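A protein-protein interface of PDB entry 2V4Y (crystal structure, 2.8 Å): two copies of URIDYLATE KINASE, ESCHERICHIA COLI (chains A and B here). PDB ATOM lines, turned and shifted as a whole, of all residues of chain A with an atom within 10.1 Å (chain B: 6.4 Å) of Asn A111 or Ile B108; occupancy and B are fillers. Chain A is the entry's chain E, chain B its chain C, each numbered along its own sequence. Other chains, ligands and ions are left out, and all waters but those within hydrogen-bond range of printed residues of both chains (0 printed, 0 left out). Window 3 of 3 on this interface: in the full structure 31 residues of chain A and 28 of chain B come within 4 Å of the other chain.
Leu A82 touches Val B85 (CD1 to CG1, 3.5 Å).
Val A85 touches Leu B82 (CG1 to CD1, 3.5 Å).
Leu A89 touches His B78 (CD2 to CB, 3.9 Å).
Leu B82 touches Leu A89 (CD1 to CD2, 3.96 Å).
Leu A110 touches Leu B110.
Ile B108 touches Asn A111.
CE1 of His B78 touches O of Gly A112 (3.6 Å).
Val A113 touches Ile B108 (CG2 to CD1, 3.9 Å).
Printed residues of chain B within 4 Å of Leu A82: Val B85.
Of the printed residues of chain B, Val A85 touches Leu B82.
Printed residues of chain B within 4 Å of Asn A111: Ile B108.
Of the printed residues of chain B, Val A113 touches Ile B108 (3.9 Å).
Of the printed residues of chain A, Val B85 touches Leu A82 (3.5 Å).
Printed residues of chain A within 4 Å of Ile B108: Asn A111 (3.999 Å) and Val A113 (3.9 Å).
Of chain A, only Pro A109 comes within 4 Å of Pro B109.
Of the printed residues of chain A, Leu B110 touches Leu A110 (3.1 Å).
No residue of chain A comes within 4 Å of Gly B139.
The nearest printed residue of chain A that does not touch Ile B108 is Leu A110 (4.2 Å).
OG of Ser B106 sits at hydrogen-bond distance from O of Ile B108.
O of Pro A109 sits close to O of Pro B109, 3.5 Å away.
Hydrophobic or aromatic side chains of chain A within 4 Å of the printed part of chain B: Leu A82, Val A85, Leu A89, Leu A110 and Val A113.
Hydrophobic or aromatic side chains of chain B that line the printed part of chain A: His B78, Leu B82, Val B85, Ile B108 and Leu B110.
Along chain B the printed residues that touch a printed residue of chain A span positions 78 to 110.
Among the printed residues, 9 pairs touch across the chains.
Among the printed residues, no Asp or Glu carboxylate lies within 4 Å of a Lys or Arg side-chain nitrogen of the other chain.
Leu A82 touches Val B85, and with the chains exchanged Val A85 touches Leu B82.
Pro A109 touches its own counterpart, Pro B109.
Leu B110 touches its own counterpart, Leu A110.
Asn A111 touches Ile B108, but with the chains exchanged Ile A108 does not touch Asn B111 (4.04 Å).
Positions printed for both chains: 82, 85, 106, 107, 108, 109, 110, 111, 114, 115, 116 and 117.
Of the 9 pairs that touch across the chains among the printed residues, 4 have their exchanged pair printed and touching as well.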
ATOM      1  N   LEU A  82      -8.087 -30.822 -16.164  1.00  0.00           N
ATOM      2  CA  LEU A  82      -8.505 -29.578 -16.795  1.00  0.00           C
ATOM      3  C   LEU A  82      -9.525 -29.879 -17.875  1.00  0.00           C
ATOM      4  O   LEU A  82     -10.479 -29.132 -18.055  1.00  0.00           O
ATOM      5  CB  LEU A  82      -7.314 -28.835 -17.388  1.00  0.00           C
ATOM      6  CG  LEU A  82      -6.272 -28.374 -16.381  1.00  0.00           C
ATOM      7  CD1 LEU A  82      -5.252 -27.477 -17.052  1.00  0.00           C
ATOM      8  CD2 LEU A  82      -6.937 -27.649 -15.232  1.00  0.00           C
ATOM      9  N   VAL A  85     -12.992 -29.920 -16.850  1.00  0.00           N
ATOM     10  CA  VAL A  85     -13.544 -28.615 -16.514  1.00  0.00           C
ATOM     11  C   VAL A  85     -14.055 -27.941 -17.770  1.00  0.00           C
ATOM     12  O   VAL A  85     -15.013 -27.186 -17.733  1.00  0.00           O
ATOM     13  CB  VAL A  85     -12.515 -27.692 -15.792  1.00  0.00           C
ATOM     14  CG1 VAL A  85     -13.169 -26.386 -15.379  1.00  0.00           C
ATOM     15  CG2 VAL A  85     -11.905 -28.391 -14.573  1.00  0.00           C
ATOM     16  N   LEU A  89     -17.742 -26.868 -18.191  1.00  0.00           N
ATOM     17  CA  LEU A  89     -17.954 -25.496 -18.616  1.00  0.00           C
ATOM     18  C   LEU A  89     -18.980 -25.471 -19.751  1.00  0.00           C
ATOM     19  O   LEU A  89     -19.910 -24.670 -19.755  1.00  0.00           O
ATOM     20  CB  LEU A  89     -16.613 -24.914 -19.077  1.00  0.00           C
ATOM     21  CG  LEU A  89     -16.151 -23.524 -18.647  1.00  0.00           C
ATOM     22  CD1 LEU A  89     -16.709 -23.137 -17.292  1.00  0.00           C
ATOM     23  CD2 LEU A  89     -14.638 -23.497 -18.628  1.00  0.00           C
ATOM     24  N   ARG A  92     -22.547 -26.610 -18.424  1.00  0.00           N
ATOM     25  CA  ARG A  92     -23.238 -25.565 -17.688  1.00  0.00           C
ATOM     26  C   ARG A  92     -23.844 -24.582 -18.667  1.00  0.00           C
ATOM     27  O   ARG A  92     -24.983 -24.161 -18.509  1.00  0.00           O
ATOM     28  CB  ARG A  92     -22.303 -24.835 -16.717  1.00  0.00           C
ATOM     29  CG  ARG A  92     -23.006 -23.750 -15.905  1.00  0.00           C
ATOM     30  CD  ARG A  92     -22.032 -22.864 -15.174  1.00  0.00           C
ATOM     31  NE  ARG A  92     -21.126 -22.149 -16.076  1.00  0.00           N
ATOM     32  CZ  ARG A  92     -20.163 -21.328 -15.660  1.00  0.00           C
ATOM     33  NH1 ARG A  92     -19.989 -21.123 -14.355  1.00  0.00           N
ATOM     34  NH2 ARG A  92     -19.377 -20.715 -16.537  1.00  0.00           N
ATOM     35  N   LEU A 104     -21.360 -24.562 -12.122  1.00  0.00           N
ATOM     36  CA  LEU A 104     -20.171 -25.385 -12.268  1.00  0.00           C
ATOM     37  C   LEU A 104     -19.256 -25.256 -11.048  1.00  0.00           C
ATOM     38  O   LEU A 104     -18.901 -24.157 -10.643  1.00  0.00           O
ATOM     39  CB  LEU A 104     -19.408 -25.008 -13.540  1.00  0.00           C
ATOM     40  CG  LEU A 104     -18.134 -25.840 -13.724  1.00  0.00           C
ATOM     41  CD1 LEU A 104     -18.479 -27.306 -13.737  1.00  0.00           C
ATOM     42  CD2 LEU A 104     -17.397 -25.469 -14.971  1.00  0.00           C
ATOM     43  N   SER A 106     -15.541 -26.776  -9.243  1.00  0.00           N
ATOM     44  CA  SER A 106     -14.287 -27.425  -9.596  1.00  0.00           C
ATOM     45  C   SER A 106     -13.528 -27.841  -8.349  1.00  0.00           C
ATOM     46  O   SER A 106     -13.460 -27.084  -7.378  1.00  0.00           O
ATOM     47  CB  SER A 106     -13.431 -26.468 -10.425  1.00  0.00           C
ATOM     48  OG  SER A 106     -12.240 -27.088 -10.859  1.00  0.00           O
ATOM     49  N   ALA A 107     -12.953 -29.037  -8.370  1.00  0.00           N
ATOM     50  CA  ALA A 107     -12.146 -29.495  -7.244  1.00  0.00           C
ATOM     51  C   ALA A 107     -10.898 -28.633  -7.099  1.00  0.00           C
ATOM     52  O   ALA A 107     -10.363 -28.460  -6.004  1.00  0.00           O
ATOM     53  CB  ALA A 107     -11.769 -30.951  -7.423  1.00  0.00           C
ATOM     54  N   ILE A 108     -10.443 -28.096  -8.227  1.00  0.00           N
ATOM     55  CA  ILE A 108      -9.350 -27.142  -8.264  1.00  0.00           C
ATOM     56  C   ILE A 108      -9.935 -25.750  -8.466  1.00  0.00           C
ATOM     57  O   ILE A 108     -10.456 -25.453  -9.535  1.00  0.00           O
ATOM     58  CB  ILE A 108      -8.426 -27.442  -9.449  1.00  0.00           C
ATOM     59  CG1 ILE A 108      -7.929 -28.883  -9.387  1.00  0.00           C
ATOM     60  CG2 ILE A 108      -7.234 -26.509  -9.459  1.00  0.00           C
ATOM     61  CD1 ILE A 108      -7.206 -29.331 -10.642  1.00  0.00           C
ATOM     62  N   PRO A 109      -9.852 -24.886  -7.447  1.00  0.00           N
ATOM     63  CA  PRO A 109     -10.402 -23.533  -7.597  1.00  0.00           C
ATOM     64  C   PRO A 109      -9.933 -22.859  -8.886  1.00  0.00           C
ATOM     65  O   PRO A 109      -8.757 -22.920  -9.233  1.00  0.00           O
ATOM     66  CB  PRO A 109      -9.846 -22.784  -6.377  1.00  0.00           C
ATOM     67  CG  PRO A 109      -9.566 -23.840  -5.394  1.00  0.00           C
ATOM     68  CD  PRO A 109      -9.129 -25.046  -6.178  1.00  0.00           C
ATOM     69  N   LEU A 110     -10.863 -22.220  -9.583  1.00  0.00           N
ATOM     70  CA  LEU A 110     -10.553 -21.512 -10.820  1.00  0.00           C
ATOM     71  C   LEU A 110     -11.115 -20.107 -10.746  1.00  0.00           C
ATOM     72  O   LEU A 110     -12.220 -19.853 -11.177  1.00  0.00           O
ATOM     73  CB  LEU A 110     -11.150 -22.242 -12.022  1.00  0.00           C
ATOM     74  CG  LEU A 110     -10.549 -23.618 -12.260  1.00  0.00           C
ATOM     75  CD1 LEU A 110     -11.419 -24.425 -13.197  1.00  0.00           C
ATOM     76  CD2 LEU A 110      -9.168 -23.434 -12.819  1.00  0.00           C
ATOM     77  N   ASN A 111     -10.344 -19.192 -10.191  1.00  0.00           N
ATOM     78  CA  ASN A 111     -10.846 -17.857  -9.939  1.00  0.00           C
ATOM     79  C   ASN A 111     -11.495 -17.248 -11.170  1.00  0.00           C
ATOM     80  O   ASN A 111     -10.871 -17.147 -12.213  1.00  0.00           O
ATOM     81  CB  ASN A 111      -9.719 -16.959  -9.428  1.00  0.00           C
ATOM     82  CG  ASN A 111     -10.211 -15.592  -9.004  1.00  0.00           C
ATOM     83  OD1 ASN A 111      -9.839 -14.571  -9.598  1.00  0.00           O
ATOM     84  ND2 ASN A 111     -11.067 -15.564  -7.981  1.00  0.00           N
ATOM     85  N   GLY A 112     -12.762 -16.857 -11.040  1.00  0.00           N
ATOM     86  CA  GLY A 112     -13.454 -16.109 -12.082  1.00  0.00           C
ATOM     87  C   GLY A 112     -14.082 -16.954 -13.180  1.00  0.00           C
ATOM     88  O   GLY A 112     -14.823 -16.446 -14.027  1.00  0.00           O
ATOM     89  N   VAL A 113     -13.796 -18.250 -13.156  1.00  0.00           N
ATOM     90  CA  VAL A 113     -14.267 -19.171 -14.181  1.00  0.00           C
ATOM     91  C   VAL A 113     -15.475 -19.956 -13.683  1.00  0.00           C
ATOM     92  O   VAL A 113     -16.444 -20.149 -14.408  1.00  0.00           O
ATOM     93  CB  VAL A 113     -13.132 -20.143 -14.623  1.00  0.00           C
ATOM     94  CG1 VAL A 113     -13.648 -21.218 -15.563  1.00  0.00           C
ATOM     95  CG2 VAL A 113     -11.993 -19.371 -15.277  1.00  0.00           C
ATOM     96  N   CYS A 114     -15.406 -20.388 -12.435  1.00  0.00           N
ATOM     97  CA  CYS A 114     -16.469 -21.142 -11.791  1.00  0.00           C
ATOM     98  C   CYS A 114     -16.140 -21.216 -10.302  1.00  0.00           C
ATOM     99  O   CYS A 114     -15.001 -20.967  -9.908  1.00  0.00           O
ATOM    100  CB  CYS A 114     -16.558 -22.539 -12.394  1.00  0.00           C
ATOM    101  SG  CYS A 114     -15.224 -23.656 -11.967  1.00  0.00           S
ATOM    102  N   ASP A 115     -17.102 -21.548  -9.457  1.00  0.00           N
ATOM    103  CA  ASP A 115     -16.782 -21.584  -8.040  1.00  0.00           C
ATOM    104  C   ASP A 115     -16.117 -22.879  -7.607  1.00  0.00           C
ATOM    105  O   ASP A 115     -16.221 -23.903  -8.285  1.00  0.00           O
ATOM    106  CB  ASP A 115     -17.956 -21.194  -7.123  1.00  0.00           C
ATOM    107  CG  ASP A 115     -19.305 -21.587  -7.674  1.00  0.00           C
ATOM    108  OD1 ASP A 115     -19.502 -21.530  -8.902  1.00  0.00           O
ATOM    109  OD2 ASP A 115     -20.191 -21.917  -6.856  1.00  0.00           O
ATOM    110  N   SER A 116     -15.398 -22.798  -6.491  1.00  0.00           N
ATOM    111  CA  SER A 116     -14.698 -23.940  -5.943  1.00  0.00           C
ATOM    112  C   SER A 116     -15.699 -24.916  -5.344  1.00  0.00           C
ATOM    113  O   SER A 116     -16.722 -24.517  -4.789  1.00  0.00           O
ATOM    114  CB  SER A 116     -13.712 -23.489  -4.866  1.00  0.00           C
ATOM    115  OG  SER A 116     -13.027 -22.312  -5.260  1.00  0.00           O
ATOM    116  N   TYR A 117     -15.398 -26.201  -5.455  1.00  0.00           N
ATOM    117  CA  TYR A 117     -16.262 -27.208  -4.885  1.00  0.00           C
ATOM    118  C   TYR A 117     -16.356 -27.064  -3.380  1.00  0.00           C
ATOM    119  O   TYR A 117     -15.372 -26.792  -2.700  1.00  0.00           O
ATOM    120  CB  TYR A 117     -15.778 -28.609  -5.215  1.00  0.00           C
ATOM    121  CG  TYR A 117     -16.605 -29.673  -4.548  1.00  0.00           C
ATOM    122  CD1 TYR A 117     -17.876 -29.966  -5.004  1.00  0.00           C
ATOM    123  CD2 TYR A 117     -16.119 -30.383  -3.467  1.00  0.00           C
ATOM    124  CE1 TYR A 117     -18.643 -30.946  -4.407  1.00  0.00           C
ATOM    125  CE2 TYR A 117     -16.879 -31.373  -2.856  1.00  0.00           C
ATOM    126  CZ  TYR A 117     -18.137 -31.653  -3.332  1.00  0.00           C
ATOM    127  OH  TYR A 117     -18.892 -32.629  -2.726  1.00  0.00           O
ATOM    128  N   HIS B  78     -13.201 -19.147 -21.886  1.00  0.00           N
ATOM    129  CA  HIS B  78     -12.702 -19.801 -20.679  1.00  0.00           C
ATOM    130  C   HIS B  78     -12.269 -21.214 -21.003  1.00  0.00           C
ATOM    131  O   HIS B  78     -11.304 -21.702 -20.442  1.00  0.00           O
ATOM    132  CB  HIS B  78     -13.736 -19.818 -19.543  1.00  0.00           C
ATOM    133  CG  HIS B  78     -13.889 -18.505 -18.846  1.00  0.00           C
ATOM    134  ND1 HIS B  78     -15.002 -18.181 -18.099  1.00  0.00           N
ATOM    135  CD2 HIS B  78     -13.073 -17.426 -18.789  1.00  0.00           C
ATOM    136  CE1 HIS B  78     -14.864 -16.961 -17.615  1.00  0.00           C
ATOM    137  NE2 HIS B  78     -13.702 -16.480 -18.019  1.00  0.00           N
ATOM    138  N   MET B  81      -9.054 -20.956 -22.664  1.00  0.00           N
ATOM    139  CA  MET B  81      -8.065 -20.572 -21.667  1.00  0.00           C
ATOM    140  C   MET B  81      -7.541 -21.816 -20.963  1.00  0.00           C
ATOM    141  O   MET B  81      -6.335 -21.994 -20.831  1.00  0.00           O
ATOM    142  CB  MET B  81      -8.705 -19.616 -20.675  1.00  0.00           C
ATOM    143  CG  MET B  81      -7.759 -18.835 -19.819  1.00  0.00           C
ATOM    144  SD  MET B  81      -8.629 -17.422 -19.098  1.00  0.00           S
ATOM    145  CE  MET B  81      -9.153 -16.600 -20.608  1.00  0.00           C
ATOM    146  N   LEU B  82      -8.449 -22.691 -20.537  1.00  0.00           N
ATOM    147  CA  LEU B  82      -8.050 -23.949 -19.926  1.00  0.00           C
ATOM    148  C   LEU B  82      -7.254 -24.782 -20.911  1.00  0.00           C
ATOM    149  O   LEU B  82      -6.274 -25.433 -20.543  1.00  0.00           O
ATOM    150  CB  LEU B  82      -9.266 -24.730 -19.437  1.00  0.00           C
ATOM    151  CG  LEU B  82     -10.073 -24.063 -18.325  1.00  0.00           C
ATOM    152  CD1 LEU B  82     -11.090 -25.032 -17.779  1.00  0.00           C
ATOM    153  CD2 LEU B  82      -9.173 -23.558 -17.211  1.00  0.00           C
ATOM    154  N   VAL B  85      -3.670 -24.164 -20.987  1.00  0.00           N
ATOM    155  CA  VAL B  85      -2.948 -24.667 -19.835  1.00  0.00           C
ATOM    156  C   VAL B  85      -2.607 -26.127 -20.030  1.00  0.00           C
ATOM    157  O   VAL B  85      -1.595 -26.595 -19.540  1.00  0.00           O
ATOM    158  CB  VAL B  85      -3.723 -24.485 -18.525  1.00  0.00           C
ATOM    159  CG1 VAL B  85      -2.898 -24.972 -17.369  1.00  0.00           C
ATOM    160  CG2 VAL B  85      -4.102 -23.012 -18.319  1.00  0.00           C
ATOM    161  N   SER B 106       0.394 -19.782 -14.786  1.00  0.00           N
ATOM    162  CA  SER B 106      -0.953 -19.623 -15.306  1.00  0.00           C
ATOM    163  C   SER B 106      -1.521 -18.295 -14.861  1.00  0.00           C
ATOM    164  O   SER B 106      -1.310 -17.877 -13.730  1.00  0.00           O
ATOM    165  CB  SER B 106      -1.838 -20.761 -14.816  1.00  0.00           C
ATOM    166  OG  SER B 106      -3.128 -20.680 -15.376  1.00  0.00           O
ATOM    167  N   ALA B 107      -2.233 -17.622 -15.753  1.00  0.00           N
ATOM    168  CA  ALA B 107      -2.870 -16.356 -15.398  1.00  0.00           C
ATOM    169  C   ALA B 107      -3.978 -16.603 -14.371  1.00  0.00           C
ATOM    170  O   ALA B 107      -4.303 -15.741 -13.551  1.00  0.00           O
ATOM    171  CB  ALA B 107      -3.426 -15.683 -16.633  1.00  0.00           C
ATOM    172  N   ILE B 108      -4.544 -17.801 -14.434  1.00  0.00           N
ATOM    173  CA  ILE B 108      -5.543 -18.250 -13.489  1.00  0.00           C
ATOM    174  C   ILE B 108      -4.874 -19.247 -12.556  1.00  0.00           C
ATOM    175  O   ILE B 108      -4.553 -20.366 -12.977  1.00  0.00           O
ATOM    176  CB  ILE B 108      -6.692 -18.990 -14.214  1.00  0.00           C
ATOM    177  CG1 ILE B 108      -7.328 -18.104 -15.280  1.00  0.00           C
ATOM    178  CG2 ILE B 108      -7.755 -19.432 -13.244  1.00  0.00           C
ATOM    179  CD1 ILE B 108      -8.242 -18.864 -16.227  1.00  0.00           C
ATOM    180  N   PRO B 109      -4.682 -18.866 -11.280  1.00  0.00           N
ATOM    181  CA  PRO B 109      -4.032 -19.777 -10.331  1.00  0.00           C
ATOM    182  C   PRO B 109      -4.644 -21.179 -10.362  1.00  0.00           C
ATOM    183  O   PRO B 109      -5.866 -21.327 -10.356  1.00  0.00           O
ATOM    184  CB  PRO B 109      -4.305 -19.129  -8.982  1.00  0.00           C
ATOM    185  CG  PRO B 109      -4.550 -17.693  -9.288  1.00  0.00           C
ATOM    186  CD  PRO B 109      -5.226 -17.671 -10.616  1.00  0.00           C
ATOM    187  N   LEU B 110      -3.793 -22.194 -10.400  1.00  0.00           N
ATOM    188  CA  LEU B 110      -4.259 -23.567 -10.398  1.00  0.00           C
ATOM    189  C   LEU B 110      -3.536 -24.331  -9.310  1.00  0.00           C
ATOM    190  O   LEU B 110      -2.492 -24.921  -9.547  1.00  0.00           O
ATOM    191  CB  LEU B 110      -3.973 -24.213 -11.739  1.00  0.00           C
ATOM    192  CG  LEU B 110      -4.724 -23.625 -12.918  1.00  0.00           C
ATOM    193  CD1 LEU B 110      -4.084 -24.069 -14.218  1.00  0.00           C
ATOM    194  CD2 LEU B 110      -6.132 -24.088 -12.852  1.00  0.00           C
ATOM    195  N   ASN B 111      -4.102 -24.316  -8.111  1.00  0.00           N
ATOM    196  CA  ASN B 111      -3.439 -24.877  -6.943  1.00  0.00           C
ATOM    197  C   ASN B 111      -2.958 -26.303  -7.185  1.00  0.00           C
ATOM    198  O   ASN B 111      -3.738 -27.176  -7.548  1.00  0.00           O
ATOM    199  CB  ASN B 111      -4.375 -24.816  -5.730  1.00  0.00           C
ATOM    200  CG  ASN B 111      -3.705 -25.266  -4.454  1.00  0.00           C
ATOM    201  OD1 ASN B 111      -4.082 -26.287  -3.865  1.00  0.00           O
ATOM    202  ND2 ASN B 111      -2.698 -24.510  -4.017  1.00  0.00           N
ATOM    203  N   CYS B 114       0.349 -25.939 -11.163  1.00  0.00           N
ATOM    204  CA  CYS B 114       1.428 -25.084 -11.633  1.00  0.00           C
ATOM    205  C   CYS B 114       1.334 -23.768 -10.870  1.00  0.00           C
ATOM    206  O   CYS B 114       0.299 -23.473 -10.278  1.00  0.00           O
ATOM    207  CB  CYS B 114       1.290 -24.839 -13.124  1.00  0.00           C
ATOM    208  SG  CYS B 114      -0.130 -23.843 -13.585  1.00  0.00           S
ATOM    209  N   ASP B 115       2.395 -22.974 -10.845  1.00  0.00           N
ATOM    210  CA  ASP B 115       2.313 -21.753 -10.055  1.00  0.00           C
ATOM    211  C   ASP B 115       1.609 -20.637 -10.790  1.00  0.00           C
ATOM    212  O   ASP B 115       1.475 -20.662 -12.003  1.00  0.00           O
ATOM    213  CB  ASP B 115       3.651 -21.290  -9.448  1.00  0.00           C
ATOM    214  CG  ASP B 115       4.850 -21.650 -10.288  1.00  0.00           C
ATOM    215  OD1 ASP B 115       4.853 -22.731 -10.917  1.00  0.00           O
ATOM    216  OD2 ASP B 115       5.816 -20.854 -10.278  1.00  0.00           O
ATOM    217  N   SER B 116       1.113 -19.683 -10.019  1.00  0.00           N
ATOM    218  CA  SER B 116       0.387 -18.560 -10.557  1.00  0.00           C
ATOM    219  C   SER B 116       1.372 -17.624 -11.230  1.00  0.00           C
ATOM    220  O   SER B 116       2.524 -17.520 -10.817  1.00  0.00           O
ATOM    221  CB  SER B 116      -0.345 -17.837  -9.427  1.00  0.00           C
ATOM    222  OG  SER B 116      -0.951 -18.773  -8.551  1.00  0.00           O
ATOM    223  N   TYR B 117       0.918 -16.946 -12.275  1.00  0.00           N
ATOM    224  CA  TYR B 117       1.768 -16.005 -12.967  1.00  0.00           C
ATOM    225  C   TYR B 117       2.137 -14.859 -12.054  1.00  0.00           C
ATOM    226  O   TYR B 117       1.335 -14.401 -11.257  1.00  0.00           O
ATOM    227  CB  TYR B 117       1.101 -15.469 -14.230  1.00  0.00           C
ATOM    228  CG  TYR B 117       1.934 -14.410 -14.903  1.00  0.00           C
ATOM    229  CD1 TYR B 117       3.059 -14.753 -15.644  1.00  0.00           C
ATOM    230  CD2 TYR B 117       1.612 -13.061 -14.786  1.00  0.00           C
ATOM    231  CE1 TYR B 117       3.842 -13.783 -16.253  1.00  0.00           C
ATOM    232  CE2 TYR B 117       2.378 -12.087 -15.393  1.00  0.00           C
ATOM    233  CZ  TYR B 117       3.495 -12.455 -16.119  1.00  0.00           C
ATOM    234  OH  TYR B 117       4.268 -11.497 -16.713  1.00  0.00           O
ATOM    235  N   SER B 135       0.644 -19.627 -19.393  1.00  0.00           N
ATOM    236  CA  SER B 135      -0.623 -20.215 -19.799  1.00  0.00           C
ATOM    237  C   SER B 135      -1.829 -19.379 -19.418  1.00  0.00           C
ATOM    238  O   SER B 135      -1.718 -18.410 -18.655  1.00  0.00           O
ATOM    239  CB  SER B 135      -0.760 -21.608 -19.199  1.00  0.00           C
ATOM    240  OG  SER B 135       0.253 -22.449 -19.714  1.00  0.00           O
ATOM    241  N   ALA B 136      -2.977 -19.776 -19.965  1.00  0.00           N
ATOM    242  CA  ALA B 136      -4.257 -19.135 -19.686  1.00  0.00           C
ATOM    243  C   ALA B 136      -4.268 -17.686 -20.142  1.00  0.00           C
ATOM    244  O   ALA B 136      -4.971 -16.849 -19.570  1.00  0.00           O
ATOM    245  CB  ALA B 136      -4.611 -19.243 -18.191  1.00  0.00           C
ATOM    246  N   GLY B 139      -5.778 -14.093 -18.800  1.00  0.00           N
ATOM    247  CA  GLY B 139      -6.655 -14.371 -17.678  1.00  0.00           C
ATOM    248  C   GLY B 139      -8.072 -13.930 -17.995  1.00  0.00           C
ATOM    249  O   GLY B 139      -9.020 -14.310 -17.308  1.00  0.00           O
ATOM    250  N   ASN B 140      -8.207 -13.128 -19.050  1.00  0.00           N
ATOM    251  CA  ASN B 140      -9.501 -12.624 -19.489  1.00  0.00           C
ATOM    252  C   ASN B 140      -9.951 -13.234 -20.803  1.00  0.00           C
ATOM    253  O   ASN B 140      -9.131 -13.731 -21.574  1.00  0.00           O
ATOM    254  CB  ASN B 140      -9.450 -11.113 -19.644  1.00  0.00           C
ATOM    255  CG  ASN B 140      -9.205 -10.418 -18.342  1.00  0.00           C
ATOM    256  OD1 ASN B 140      -9.956 -10.592 -17.381  1.00  0.00           O
ATOM    257  ND2 ASN B 140      -8.146  -9.622 -18.293  1.00  0.00           N
